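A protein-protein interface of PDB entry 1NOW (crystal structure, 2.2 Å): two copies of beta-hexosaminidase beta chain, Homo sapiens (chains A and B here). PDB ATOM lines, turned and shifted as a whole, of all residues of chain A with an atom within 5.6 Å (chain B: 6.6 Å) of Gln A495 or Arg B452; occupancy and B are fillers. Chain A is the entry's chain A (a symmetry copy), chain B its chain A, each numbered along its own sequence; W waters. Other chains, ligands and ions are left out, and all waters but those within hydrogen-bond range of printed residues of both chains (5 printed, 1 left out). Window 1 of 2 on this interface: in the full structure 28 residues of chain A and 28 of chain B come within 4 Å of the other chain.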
ATOM      1  N   THR A 450      21.913  22.239  -3.363  1.00  0.00           N
ATOM      2  CA  THR A 450      21.055  21.371  -4.166  1.00  0.00           C
ATOM      3  C   THR A 450      19.564  21.544  -3.940  1.00  0.00           C
ATOM      4  O   THR A 450      18.847  21.744  -4.918  1.00  0.00           O
ATOM      5  CB  THR A 450      21.543  19.924  -4.036  1.00  0.00           C
ATOM      6  OG1 THR A 450      22.812  19.844  -4.674  1.00  0.00           O
ATOM      7  CG2 THR A 450      20.685  18.934  -4.816  1.00  0.00           C
ATOM      8  N   PRO A 451      19.087  21.477  -2.697  1.00  0.00           N
ATOM      9  CA  PRO A 451      17.668  21.723  -2.435  1.00  0.00           C
ATOM     10  C   PRO A 451      17.255  23.122  -2.847  1.00  0.00           C
ATOM     11  O   PRO A 451      16.139  23.279  -3.301  1.00  0.00           O
ATOM     12  CB  PRO A 451      17.535  21.604  -0.915  1.00  0.00           C
ATOM     13  CG  PRO A 451      18.866  21.245  -0.380  1.00  0.00           C
ATOM     14  CD  PRO A 451      19.823  21.166  -1.457  1.00  0.00           C
ATOM     15  N   ARG A 452      18.119  24.120  -2.692  1.00  0.00           N
ATOM     16  CA  ARG A 452      17.757  25.457  -3.137  1.00  0.00           C
ATOM     17  C   ARG A 452      17.649  25.539  -4.662  1.00  0.00           C
ATOM     18  O   ARG A 452      16.738  26.190  -5.170  1.00  0.00           O
ATOM     19  CB  ARG A 452      18.763  26.495  -2.671  1.00  0.00           C
ATOM     20  CG  ARG A 452      18.266  27.931  -2.830  1.00  0.00           C
ATOM     21  CD  ARG A 452      18.905  28.914  -1.860  1.00  0.00           C
ATOM     22  NE  ARG A 452      18.514  28.633  -0.484  1.00  0.00           N
ATOM     23  CZ  ARG A 452      19.001  29.244   0.590  1.00  0.00           C
ATOM     24  NH1 ARG A 452      19.910  30.216   0.486  1.00  0.00           N
ATOM     25  NH2 ARG A 452      18.568  28.887   1.787  1.00  0.00           N
ATOM     26  N   TRP A 454      17.275  22.922  -7.070  1.00  0.00           N
ATOM     27  CA  TRP A 454      16.341  22.030  -7.726  1.00  0.00           C
ATOM     28  C   TRP A 454      15.175  21.725  -6.817  1.00  0.00           C
ATOM     29  O   TRP A 454      15.392  21.488  -5.618  1.00  0.00           O
ATOM     30  CB  TRP A 454      17.052  20.723  -8.084  1.00  0.00           C
ATOM     31  CG  TRP A 454      18.329  20.945  -8.846  1.00  0.00           C
ATOM     32  CD1 TRP A 454      19.590  20.799  -8.368  1.00  0.00           C
ATOM     33  CD2 TRP A 454      18.463  21.334 -10.209  1.00  0.00           C
ATOM     34  NE1 TRP A 454      20.508  21.085  -9.346  1.00  0.00           N
ATOM     35  CE2 TRP A 454      19.843  21.411 -10.491  1.00  0.00           C
ATOM     36  CE3 TRP A 454      17.561  21.617 -11.235  1.00  0.00           C
ATOM     37  CZ2 TRP A 454      20.333  21.764 -11.738  1.00  0.00           C
ATOM     38  CZ3 TRP A 454      18.054  21.949 -12.473  1.00  0.00           C
ATOM     39  CH2 TRP A 454      19.422  22.035 -12.713  1.00  0.00           C
ATOM     40  N   PRO A 455      13.938  21.696  -7.321  1.00  0.00           N
ATOM     41  CA  PRO A 455      13.540  21.870  -8.716  1.00  0.00           C
ATOM     42  C   PRO A 455      13.189  23.296  -9.165  1.00  0.00           C
ATOM     43  O   PRO A 455      12.569  23.425 -10.226  1.00  0.00           O
ATOM     44  CB  PRO A 455      12.292  21.011  -8.765  1.00  0.00           C
ATOM     45  CG  PRO A 455      11.622  21.341  -7.470  1.00  0.00           C
ATOM     46  CD  PRO A 455      12.770  21.447  -6.475  1.00  0.00           C
ATOM     47  N   ARG A 456      13.528  24.334  -8.402  1.00  0.00           N
ATOM     48  CA  ARG A 456      13.224  25.696  -8.849  1.00  0.00           C
ATOM     49  C   ARG A 456      13.827  25.967 -10.230  1.00  0.00           C
ATOM     50  O   ARG A 456      13.134  26.496 -11.103  1.00  0.00           O
ATOM     51  CB  ARG A 456      13.653  26.751  -7.816  1.00  0.00           C
ATOM     52  CG  ARG A 456      12.733  26.776  -6.581  1.00  0.00           C
ATOM     53  CD  ARG A 456      12.908  27.974  -5.667  1.00  0.00           C
ATOM     54  NE  ARG A 456      14.282  28.149  -5.371  1.00  0.00           N
ATOM     55  CZ  ARG A 456      14.953  29.279  -5.288  1.00  0.00           C
ATOM     56  NH1 ARG A 456      14.421  30.502  -5.401  1.00  0.00           N
ATOM     57  NH2 ARG A 456      16.227  29.147  -5.036  1.00  0.00           N
ATOM     58  N   ARG A 484      10.691  15.818 -10.014  1.00  0.00           N
ATOM     59  CA  ARG A 484      11.402  16.040  -8.763  1.00  0.00           C
ATOM     60  C   ARG A 484      11.637  14.731  -8.002  1.00  0.00           C
ATOM     61  O   ARG A 484      12.713  14.530  -7.465  1.00  0.00           O
ATOM     62  CB  ARG A 484      10.634  17.061  -7.921  1.00  0.00           C
ATOM     63  CG  ARG A 484      11.228  17.358  -6.604  1.00  0.00           C
ATOM     64  CD  ARG A 484      10.537  16.652  -5.495  1.00  0.00           C
ATOM     65  NE  ARG A 484      11.310  16.672  -4.268  1.00  0.00           N
ATOM     66  CZ  ARG A 484      10.898  16.178  -3.115  1.00  0.00           C
ATOM     67  NH1 ARG A 484       9.701  15.609  -3.001  1.00  0.00           N
ATOM     68  NH2 ARG A 484      11.700  16.250  -2.065  1.00  0.00           N
ATOM     69  N   ALA A 493      19.135  15.752  -4.233  1.00  0.00           N
ATOM     70  CA  ALA A 493      18.194  16.073  -3.155  1.00  0.00           C
ATOM     71  C   ALA A 493      17.366  17.311  -3.461  1.00  0.00           C
ATOM     72  O   ALA A 493      17.470  18.316  -2.768  1.00  0.00           O
ATOM     73  CB  ALA A 493      18.940  16.227  -1.818  1.00  0.00           C
ATOM     74  N   ALA A 494      16.526  17.218  -4.492  1.00  0.00           N
ATOM     75  CA  ALA A 494      15.654  18.310  -4.887  1.00  0.00           C
ATOM     76  C   ALA A 494      14.527  18.426  -3.861  1.00  0.00           C
ATOM     77  O   ALA A 494      13.973  17.412  -3.401  1.00  0.00           O
ATOM     78  CB  ALA A 494      15.103  18.063  -6.269  1.00  0.00           C
ATOM     79  N   GLN A 495      14.193  19.659  -3.501  1.00  0.00           N
ATOM     80  CA  GLN A 495      13.194  19.929  -2.465  1.00  0.00           C
ATOM     81  C   GLN A 495      11.745  19.756  -2.949  1.00  0.00           C
ATOM     82  O   GLN A 495      11.507  19.716  -4.155  1.00  0.00           O
ATOM     83  CB  GLN A 495      13.435  21.321  -1.859  1.00  0.00           C
ATOM     84  CG  GLN A 495      13.141  22.499  -2.751  1.00  0.00           C
ATOM     85  CD  GLN A 495      13.423  23.835  -2.089  1.00  0.00           C
ATOM     86  OE1 GLN A 495      13.783  23.916  -0.893  1.00  0.00           O
ATOM     87  NE2 GLN A 495      13.218  24.898  -2.848  1.00  0.00           N
ATOM     88  N   PRO A 496      10.771  19.655  -2.040  1.00  0.00           N
ATOM     89  CA  PRO A 496       9.381  19.506  -2.473  1.00  0.00           C
ATOM     90  C   PRO A 496       8.793  20.735  -3.147  1.00  0.00           C
ATOM     91  O   PRO A 496       9.277  21.839  -2.938  1.00  0.00           O
ATOM     92  CB  PRO A 496       8.619  19.285  -1.169  1.00  0.00           C
ATOM     93  CG  PRO A 496       9.632  18.981  -0.162  1.00  0.00           C
ATOM     94  CD  PRO A 496      10.873  19.634  -0.571  1.00  0.00           C
ATOM     95  N   LEU A 497       7.760  20.519  -3.953  1.00  0.00           N
ATOM     96  CA  LEU A 497       6.980  21.617  -4.515  1.00  0.00           C
ATOM     97  C   LEU A 497       5.887  22.000  -3.533  1.00  0.00           C
ATOM     98  O   LEU A 497       5.537  23.165  -3.443  1.00  0.00           O
ATOM     99  CB  LEU A 497       6.332  21.250  -5.853  1.00  0.00           C
ATOM    100  CG  LEU A 497       7.183  21.087  -7.116  1.00  0.00           C
ATOM    101  CD1 LEU A 497       6.286  21.017  -8.323  1.00  0.00           C
ATOM    102  CD2 LEU A 497       8.171  22.204  -7.337  1.00  0.00           C
ATOM    103  N   LEU B 402       9.697  29.877  10.919  1.00  0.00           N
ATOM    104  CA  LEU B 402      10.879  29.636  10.103  1.00  0.00           C
ATOM    105  C   LEU B 402      10.548  29.020   8.745  1.00  0.00           C
ATOM    106  O   LEU B 402      11.390  29.023   7.878  1.00  0.00           O
ATOM    107  CB  LEU B 402      11.928  28.779  10.834  1.00  0.00           C
ATOM    108  CG  LEU B 402      12.518  29.204  12.196  1.00  0.00           C
ATOM    109  CD1 LEU B 402      13.989  28.805  12.294  1.00  0.00           C
ATOM    110  CD2 LEU B 402      12.351  30.669  12.537  1.00  0.00           C
ATOM    111  N   ASP B 403       9.350  28.477   8.562  1.00  0.00           N
ATOM    112  CA  ASP B 403       8.929  28.070   7.227  1.00  0.00           C
ATOM    113  C   ASP B 403       8.808  29.268   6.251  1.00  0.00           C
ATOM    114  O   ASP B 403       8.984  29.102   5.035  1.00  0.00           O
ATOM    115  CB  ASP B 403       7.636  27.256   7.298  1.00  0.00           C
ATOM    116  CG  ASP B 403       6.462  28.044   7.840  1.00  0.00           C
ATOM    117  OD1 ASP B 403       6.605  28.756   8.879  1.00  0.00           O
ATOM    118  OD2 ASP B 403       5.345  27.983   7.291  1.00  0.00           O
ATOM    119  N   LEU B 404       8.552  30.467   6.782  1.00  0.00           N
ATOM    120  CA  LEU B 404       8.441  31.684   5.982  1.00  0.00           C
ATOM    121  C   LEU B 404       9.837  32.249   5.707  1.00  0.00           C
ATOM    122  O   LEU B 404      10.300  33.198   6.349  1.00  0.00           O
ATOM    123  CB  LEU B 404       7.548  32.725   6.682  1.00  0.00           C
ATOM    124  CG  LEU B 404       6.146  32.273   7.144  1.00  0.00           C
ATOM    125  CD1 LEU B 404       5.393  33.419   7.862  1.00  0.00           C
ATOM    126  CD2 LEU B 404       5.300  31.750   6.027  1.00  0.00           C
ATOM    127  N   ILE B 405      10.491  31.635   4.729  1.00  0.00           N
ATOM    128  CA  ILE B 405      11.835  32.003   4.297  1.00  0.00           C
ATOM    129  C   ILE B 405      11.861  33.305   3.502  1.00  0.00           C
ATOM    130  O   ILE B 405      10.877  33.698   2.901  1.00  0.00           O
ATOM    131  CB  ILE B 405      12.487  30.851   3.453  1.00  0.00           C
ATOM    132  CG1 ILE B 405      11.640  30.495   2.205  1.00  0.00           C
ATOM    133  CG2 ILE B 405      12.717  29.628   4.345  1.00  0.00           C
ATOM    134  CD1 ILE B 405      12.323  29.622   1.181  1.00  0.00           C
ATOM    135  N   LEU B 439       8.614  25.227  12.174  1.00  0.00           N
ATOM    136  CA  LEU B 439       8.952  24.814  10.828  1.00  0.00           C
ATOM    137  C   LEU B 439       7.838  23.967  10.230  1.00  0.00           C
ATOM    138  O   LEU B 439       7.923  22.730  10.179  1.00  0.00           O
ATOM    139  CB  LEU B 439      10.289  24.052  10.788  1.00  0.00           C
ATOM    140  CG  LEU B 439      10.847  23.844   9.366  1.00  0.00           C
ATOM    141  CD1 LEU B 439      11.178  25.162   8.693  1.00  0.00           C
ATOM    142  CD2 LEU B 439      12.098  23.001   9.401  1.00  0.00           C
ATOM    143  N   TYR B 443       6.493  22.924   2.533  1.00  0.00           N
ATOM    144  CA  TYR B 443       7.623  22.991   1.624  1.00  0.00           C
ATOM    145  C   TYR B 443       8.879  22.361   2.205  1.00  0.00           C
ATOM    146  O   TYR B 443       9.975  22.577   1.668  1.00  0.00           O
ATOM    147  CB  TYR B 443       7.845  24.459   1.267  1.00  0.00           C
ATOM    148  CG  TYR B 443       6.568  25.054   0.710  1.00  0.00           C
ATOM    149  CD1 TYR B 443       6.128  24.705  -0.557  1.00  0.00           C
ATOM    150  CD2 TYR B 443       5.758  25.886   1.478  1.00  0.00           C
ATOM    151  CE1 TYR B 443       4.955  25.201  -1.065  1.00  0.00           C
ATOM    152  CE2 TYR B 443       4.568  26.405   0.964  1.00  0.00           C
ATOM    153  CZ  TYR B 443       4.172  26.047  -0.306  1.00  0.00           C
ATOM    154  OH  TYR B 443       3.003  26.508  -0.872  1.00  0.00           O
ATOM    155  N   VAL B 444       8.721  21.541   3.244  1.00  0.00           N
ATOM    156  CA  VAL B 444       9.868  20.952   3.940  1.00  0.00           C
ATOM    157  C   VAL B 444       9.801  19.432   4.077  1.00  0.00           C
ATOM    158  O   VAL B 444       8.784  18.889   4.513  1.00  0.00           O
ATOM    159  CB  VAL B 444      10.031  21.559   5.357  1.00  0.00           C
ATOM    160  CG1 VAL B 444      11.077  20.833   6.176  1.00  0.00           C
ATOM    161  CG2 VAL B 444      10.409  23.027   5.273  1.00  0.00           C
ATOM    162  N   ASP B 445      10.894  18.755   3.729  1.00  0.00           N
ATOM    163  CA  ASP B 445      11.013  17.324   4.006  1.00  0.00           C
ATOM    164  C   ASP B 445      12.481  17.011   4.314  1.00  0.00           C
ATOM    165  O   ASP B 445      13.260  17.942   4.567  1.00  0.00           O
ATOM    166  CB  ASP B 445      10.385  16.473   2.889  1.00  0.00           C
ATOM    167  CG  ASP B 445      11.205  16.424   1.619  1.00  0.00           C
ATOM    168  OD1 ASP B 445      12.223  17.127   1.466  1.00  0.00           O
ATOM    169  OD2 ASP B 445      10.847  15.707   0.678  1.00  0.00           O
ATOM    170  N   THR B 447      14.986  16.393   2.483  1.00  0.00           N
ATOM    171  CA  THR B 447      15.968  16.982   1.575  1.00  0.00           C
ATOM    172  C   THR B 447      16.394  18.379   2.002  1.00  0.00           C
ATOM    173  O   THR B 447      17.500  18.796   1.678  1.00  0.00           O
ATOM    174  CB  THR B 447      15.444  17.077   0.125  1.00  0.00           C
ATOM    175  OG1 THR B 447      14.284  17.917   0.080  1.00  0.00           O
ATOM    176  CG2 THR B 447      14.991  15.720  -0.429  1.00  0.00           C
ATOM    177  N   ASN B 448      15.530  19.103   2.714  1.00  0.00           N
ATOM    178  CA  ASN B 448      15.824  20.494   3.055  1.00  0.00           C
ATOM    179  C   ASN B 448      15.574  20.962   4.491  1.00  0.00           C
ATOM    180  O   ASN B 448      15.817  22.131   4.797  1.00  0.00           O
ATOM    181  CB  ASN B 448      15.086  21.388   2.048  1.00  0.00           C
ATOM    182  CG  ASN B 448      13.580  21.442   2.265  1.00  0.00           C
ATOM    183  OD1 ASN B 448      13.009  20.656   3.020  1.00  0.00           O
ATOM    184  ND2 ASN B 448      12.928  22.375   1.582  1.00  0.00           N
ATOM    185  N   LEU B 449      15.121  20.069   5.371  1.00  0.00           N
ATOM    186  CA  LEU B 449      14.746  20.467   6.728  1.00  0.00           C
ATOM    187  C   LEU B 449      15.893  21.106   7.502  1.00  0.00           C
ATOM    188  O   LEU B 449      15.763  22.203   8.010  1.00  0.00           O
ATOM    189  CB  LEU B 449      14.201  19.265   7.504  1.00  0.00           C
ATOM    190  CG  LEU B 449      13.688  19.537   8.936  1.00  0.00           C
ATOM    191  CD1 LEU B 449      12.465  18.704   9.223  1.00  0.00           C
ATOM    192  CD2 LEU B 449      14.708  19.257   9.989  1.00  0.00           C
ATOM    193  N   THR B 450      17.012  20.408   7.571  1.00  0.00           N
ATOM    194  CA  THR B 450      18.131  20.821   8.415  1.00  0.00           C
ATOM    195  C   THR B 450      18.758  22.155   8.054  1.00  0.00           C
ATOM    196  O   THR B 450      18.876  23.001   8.938  1.00  0.00           O
ATOM    197  CB  THR B 450      19.134  19.667   8.517  1.00  0.00           C
ATOM    198  OG1 THR B 450      18.509  18.624   9.255  1.00  0.00           O
ATOM    199  CG2 THR B 450      20.359  20.016   9.355  1.00  0.00           C
ATOM    200  N   PRO B 451      19.153  22.366   6.797  1.00  0.00           N
ATOM    201  CA  PRO B 451      19.684  23.670   6.397  1.00  0.00           C
ATOM    202  C   PRO B 451      18.662  24.773   6.585  1.00  0.00           C
ATOM    203  O   PRO B 451      19.060  25.869   6.927  1.00  0.00           O
ATOM    204  CB  PRO B 451      19.969  23.520   4.901  1.00  0.00           C
ATOM    205  CG  PRO B 451      19.642  22.129   4.523  1.00  0.00           C
ATOM    206  CD  PRO B 451      19.141  21.412   5.671  1.00  0.00           C
ATOM    207  N   ARG B 452      17.379  24.506   6.364  1.00  0.00           N
ATOM    208  CA  ARG B 452      16.381  25.541   6.597  1.00  0.00           C
ATOM    209  C   ARG B 452      16.249  25.878   8.085  1.00  0.00           C
ATOM    210  O   ARG B 452      16.115  27.050   8.430  1.00  0.00           O
ATOM    211  CB  ARG B 452      15.016  25.130   6.075  1.00  0.00           C
ATOM    212  CG  ARG B 452      14.024  26.290   6.002  1.00  0.00           C
ATOM    213  CD  ARG B 452      12.930  26.100   4.960  1.00  0.00           C
ATOM    214  NE  ARG B 452      13.476  26.111   3.608  1.00  0.00           N
ATOM    215  CZ  ARG B 452      12.787  25.854   2.503  1.00  0.00           C
ATOM    216  NH1 ARG B 452      11.483  25.570   2.545  1.00  0.00           N
ATOM    217  NH2 ARG B 452      13.406  25.888   1.334  1.00  0.00           N
ATOM    218  N   LEU B 453      16.323  24.856   8.942  1.00  0.00           N
ATOM    219  CA  LEU B 453      16.122  25.028  10.378  1.00  0.00           C
ATOM    220  C   LEU B 453      17.293  25.714  11.057  1.00  0.00           C
ATOM    221  O   LEU B 453      17.093  26.647  11.840  1.00  0.00           O
ATOM    222  CB  LEU B 453      15.886  23.681  11.107  1.00  0.00           C
ATOM    223  CG  LEU B 453      14.772  23.508  12.152  1.00  0.00           C
ATOM    224  CD1 LEU B 453      14.969  22.286  12.971  1.00  0.00           C
ATOM    225  CD2 LEU B 453      14.509  24.695  13.032  1.00  0.00           C
ATOM    226  N   TRP B 454      18.499  25.222  10.786  1.00  0.00           N
ATOM    227  CA  TRP B 454      19.688  25.669  11.482  1.00  0.00           C
ATOM    228  C   TRP B 454      20.613  26.396  10.535  1.00  0.00           C
ATOM    229  O   TRP B 454      20.798  25.931   9.399  1.00  0.00           O
ATOM    230  CB  TRP B 454      20.420  24.459  12.065  1.00  0.00           C
ATOM    231  CG  TRP B 454      19.523  23.574  12.886  1.00  0.00           C
ATOM    232  CD1 TRP B 454      19.043  22.357  12.531  1.00  0.00           C
ATOM    233  CD2 TRP B 454      19.015  23.836  14.191  1.00  0.00           C
ATOM    234  NE1 TRP B 454      18.256  21.842  13.528  1.00  0.00           N
ATOM    235  CE2 TRP B 454      18.226  22.728  14.566  1.00  0.00           C
ATOM    236  CE3 TRP B 454      19.153  24.887  15.097  1.00  0.00           C
ATOM    237  CZ2 TRP B 454      17.579  22.650  15.787  1.00  0.00           C
ATOM    238  CZ3 TRP B 454      18.522  24.795  16.314  1.00  0.00           C
ATOM    239  CH2 TRP B 454      17.735  23.697  16.644  1.00  0.00           C
ATOM    240  N   PRO B 455      21.228  27.510  10.941  1.00  0.00           N
ATOM    241  CA  PRO B 455      21.173  28.125  12.266  1.00  0.00           C
ATOM    242  C   PRO B 455      20.094  29.193  12.491  1.00  0.00           C
ATOM    243  O   PRO B 455      20.217  29.931  13.475  1.00  0.00           O
ATOM    244  CB  PRO B 455      22.541  28.776  12.333  1.00  0.00           C
ATOM    245  CG  PRO B 455      22.698  29.340  10.959  1.00  0.00           C
ATOM    246  CD  PRO B 455      22.099  28.275  10.049  1.00  0.00           C
ATOM    247  N   ARG B 456      19.090  29.316  11.625  1.00  0.00           N
ATOM    248  CA  ARG B 456      18.043  30.312  11.860  1.00  0.00           C
ATOM    249  C   ARG B 456      17.397  30.115  13.235  1.00  0.00           C
ATOM    250  O   ARG B 456      17.229  31.088  13.973  1.00  0.00           O
ATOM    251  CB  ARG B 456      16.999  30.329  10.731  1.00  0.00           C
ATOM    252  CG  ARG B 456      17.539  30.966   9.437  1.00  0.00           C
ATOM    253  CD  ARG B 456      16.493  31.288   8.387  1.00  0.00           C
ATOM    254  NE  ARG B 456      15.668  30.156   8.177  1.00  0.00           N
ATOM    255  CZ  ARG B 456      14.363  30.130   7.994  1.00  0.00           C
ATOM    256  NH1 ARG B 456      13.576  31.209   7.901  1.00  0.00           N
ATOM    257  NH2 ARG B 456      13.848  28.938   7.861  1.00  0.00           N
ATOM    258  N   ALA B 457      17.105  28.862  13.598  1.00  0.00           N
ATOM    259  CA  ALA B 457      16.552  28.555  14.923  1.00  0.00           C
ATOM    260  C   ALA B 457      17.505  28.845  16.090  1.00  0.00           C
ATOM    261  O   ALA B 457      17.045  29.056  17.225  1.00  0.00           O
ATOM    262  CB  ALA B 457      16.085  27.117  14.986  1.00  0.00           C
ATOM    263  N   ALA B 493      23.921  19.688   9.086  1.00  0.00           N
ATOM    264  CA  ALA B 493      24.206  20.511   7.905  1.00  0.00           C
ATOM    265  C   ALA B 493      23.543  21.877   7.978  1.00  0.00           C
ATOM    266  O   ALA B 493      22.680  22.193   7.168  1.00  0.00           O
ATOM    267  CB  ALA B 493      23.799  19.767   6.621  1.00  0.00           C
ATOM    268  N   GLN B 495      23.138  25.768   7.460  1.00  0.00           N
ATOM    269  CA  GLN B 495      23.494  26.620   6.323  1.00  0.00           C
ATOM    270  C   GLN B 495      24.341  27.842   6.714  1.00  0.00           C
ATOM    271  O   GLN B 495      24.405  28.188   7.892  1.00  0.00           O
ATOM    272  CB  GLN B 495      22.224  27.023   5.557  1.00  0.00           C
ATOM    273  CG  GLN B 495      21.295  27.980   6.258  1.00  0.00           C
ATOM    274  CD  GLN B 495      20.056  28.313   5.446  1.00  0.00           C
ATOM    275  OE1 GLN B 495      19.896  27.884   4.281  1.00  0.00           O
ATOM    276  NE2 GLN B 495      19.190  29.117   6.038  1.00  0.00           N
HETATM  277  O   HOH W   1       8.573  14.355  -0.573  1.00  0.00           O
HETATM  278  O   HOH W   2      16.038  24.750   0.140  1.00  0.00           O
HETATM  279  O   HOH W   3      16.057  27.548  -0.134  1.00  0.00           O
HETATM  280  O   HOH W   4      15.683  27.634   3.219  1.00  0.00           O
HETATM  281  O   HOH W   5      18.114  26.225   3.322  1.00  0.00           O
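The side-chain amide nitrogen (ND2) of Asn B448 sits at hydrogen-bond distance from the backbone carbonyl oxygen (O) of Tyr B443, at 3.0 Å.
The backbone NH (N) of Asp B445 sits at hydrogen-bond distance from the side-chain amide oxygen (OD1) of Asn B448 (2.9 Å).
The backbone NH of Gln B495 is in hydrogen-bond range of the backbone carbonyl oxygen of Trp B454 (3.0 Å).
The backbone carbonyl oxygen of Pro A451 lies close to the side-chain amide nitrogen of Gln A495 (3.4 Å).
O of Arg A452 lies within hydrogen-bond range of NH2 of Arg A456 (3.0 Å).
The backbone carbonyl oxygen of Trp A454 is in hydrogen-bond range of the backbone NH of Gln A495 (3.0 Å).
Hydrophobic or aromatic side chains of chain B that line the printed part of chain A: Tyr B443.
Printed residues of chain A that touch a printed residue of chain B: Pro A451, Arg A452, Arg A484, Ala A493, Ala A494, Gln A495, Pro A496 and Leu A497.
Among the printed residues, 14 pairs touch across the chains.
Among the printed residues, Asp or Glu carboxylates within 4 Å of a Lys or Arg side-chain nitrogen of the other chain: Arg A484 with Asp B445 (2.9 Å).
Among the printed residues, merely in contact across the chains: Leu A497 with Tyr B443 (3.2 Å), Gln A495 with Thr B447 (3.4 Å), Pro A451 with Thr B447 (3.5 Å), Pro A496 with Asp B445 (3.5 Å), Ala A494 with Thr B447 (3.5 Å), Arg A484 with Thr B447 (3.7 Å), Ala A493 with Thr B447 (3.7 Å), Pro A496 with Tyr B443 (3.8 Å), Pro A451 with Asn B448 (3.9 Å) and Pro A496 with Thr B447 (3.9 Å).
Of the printed residues of chain B, Arg A484 touches Asp B445 (2.9 Å) and Thr B447 (3.7 Å).
Of chain B, only Thr B447 (3.4 Å), Asn B448 (3.0 Å) and Arg B452 (3.0 Å) come within 4 Å of Gln A495.
Printed residues of chain B within 4 Å of Pro A496: Tyr B443, Asp B445 and Thr B447.
Of the printed residues of chain B, Leu A497 touches Tyr B443 (3.2 Å).
Arg B452 touches just one residue of chain A: Gln A495 (3.0 Å).
Of the printed residues of chain A, Gln B495 touches Arg A452 (3.0 Å).
Water W2 lies within hydrogen-bond range of the side-chain amide oxygen of Gln A495 (2.6 Å) and the guanidinium group of Arg B452 (3.1 Å).
Water W5 lies within hydrogen-bond range of OE1 of Gln B495 (2.6 Å) and NH2 of Arg A452 (3.1 Å).
Water W3 bridges NE of Arg A452 (2.7 Å) and NH2 of Arg B452 (3.5 Å).
Water W4 bridges NE of Arg B452 (2.7 Å) and NH2 of Arg A452 (3.5 Å).
Water W1 lies within hydrogen-bond range of the side-chain carboxylate of Asp B445 (2.9 Å) and the guanidinium group of Arg A484 (3.0 Å).
Arg A452 touches Gln B495, and with the chains exchanged Gln A495 touches Arg B452.
Positions printed for both chains: 450, 451, 452, 454, 455, 456, 493 and 495.
The side-chain carboxylate (OD2) of Asp B445 lies within salt-bridge range of the guanidinium group (NH2) of Arg A484 (2.9 Å).
The side-chain amide nitrogen (ND2) of Asn B448 is in hydrogen-bond range of the side-chain amide oxygen (OE1) of Gln A495, 3.0 Å away.
The side-chain amide oxygen (OE1) of Gln A495 is in hydrogen-bond range of the guanidinium group (NH2) of Arg B452 (3.0 Å).
NH2 of Arg A452 sits at hydrogen-bond distance from OE1 of Gln B495, 3.0 Å away.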
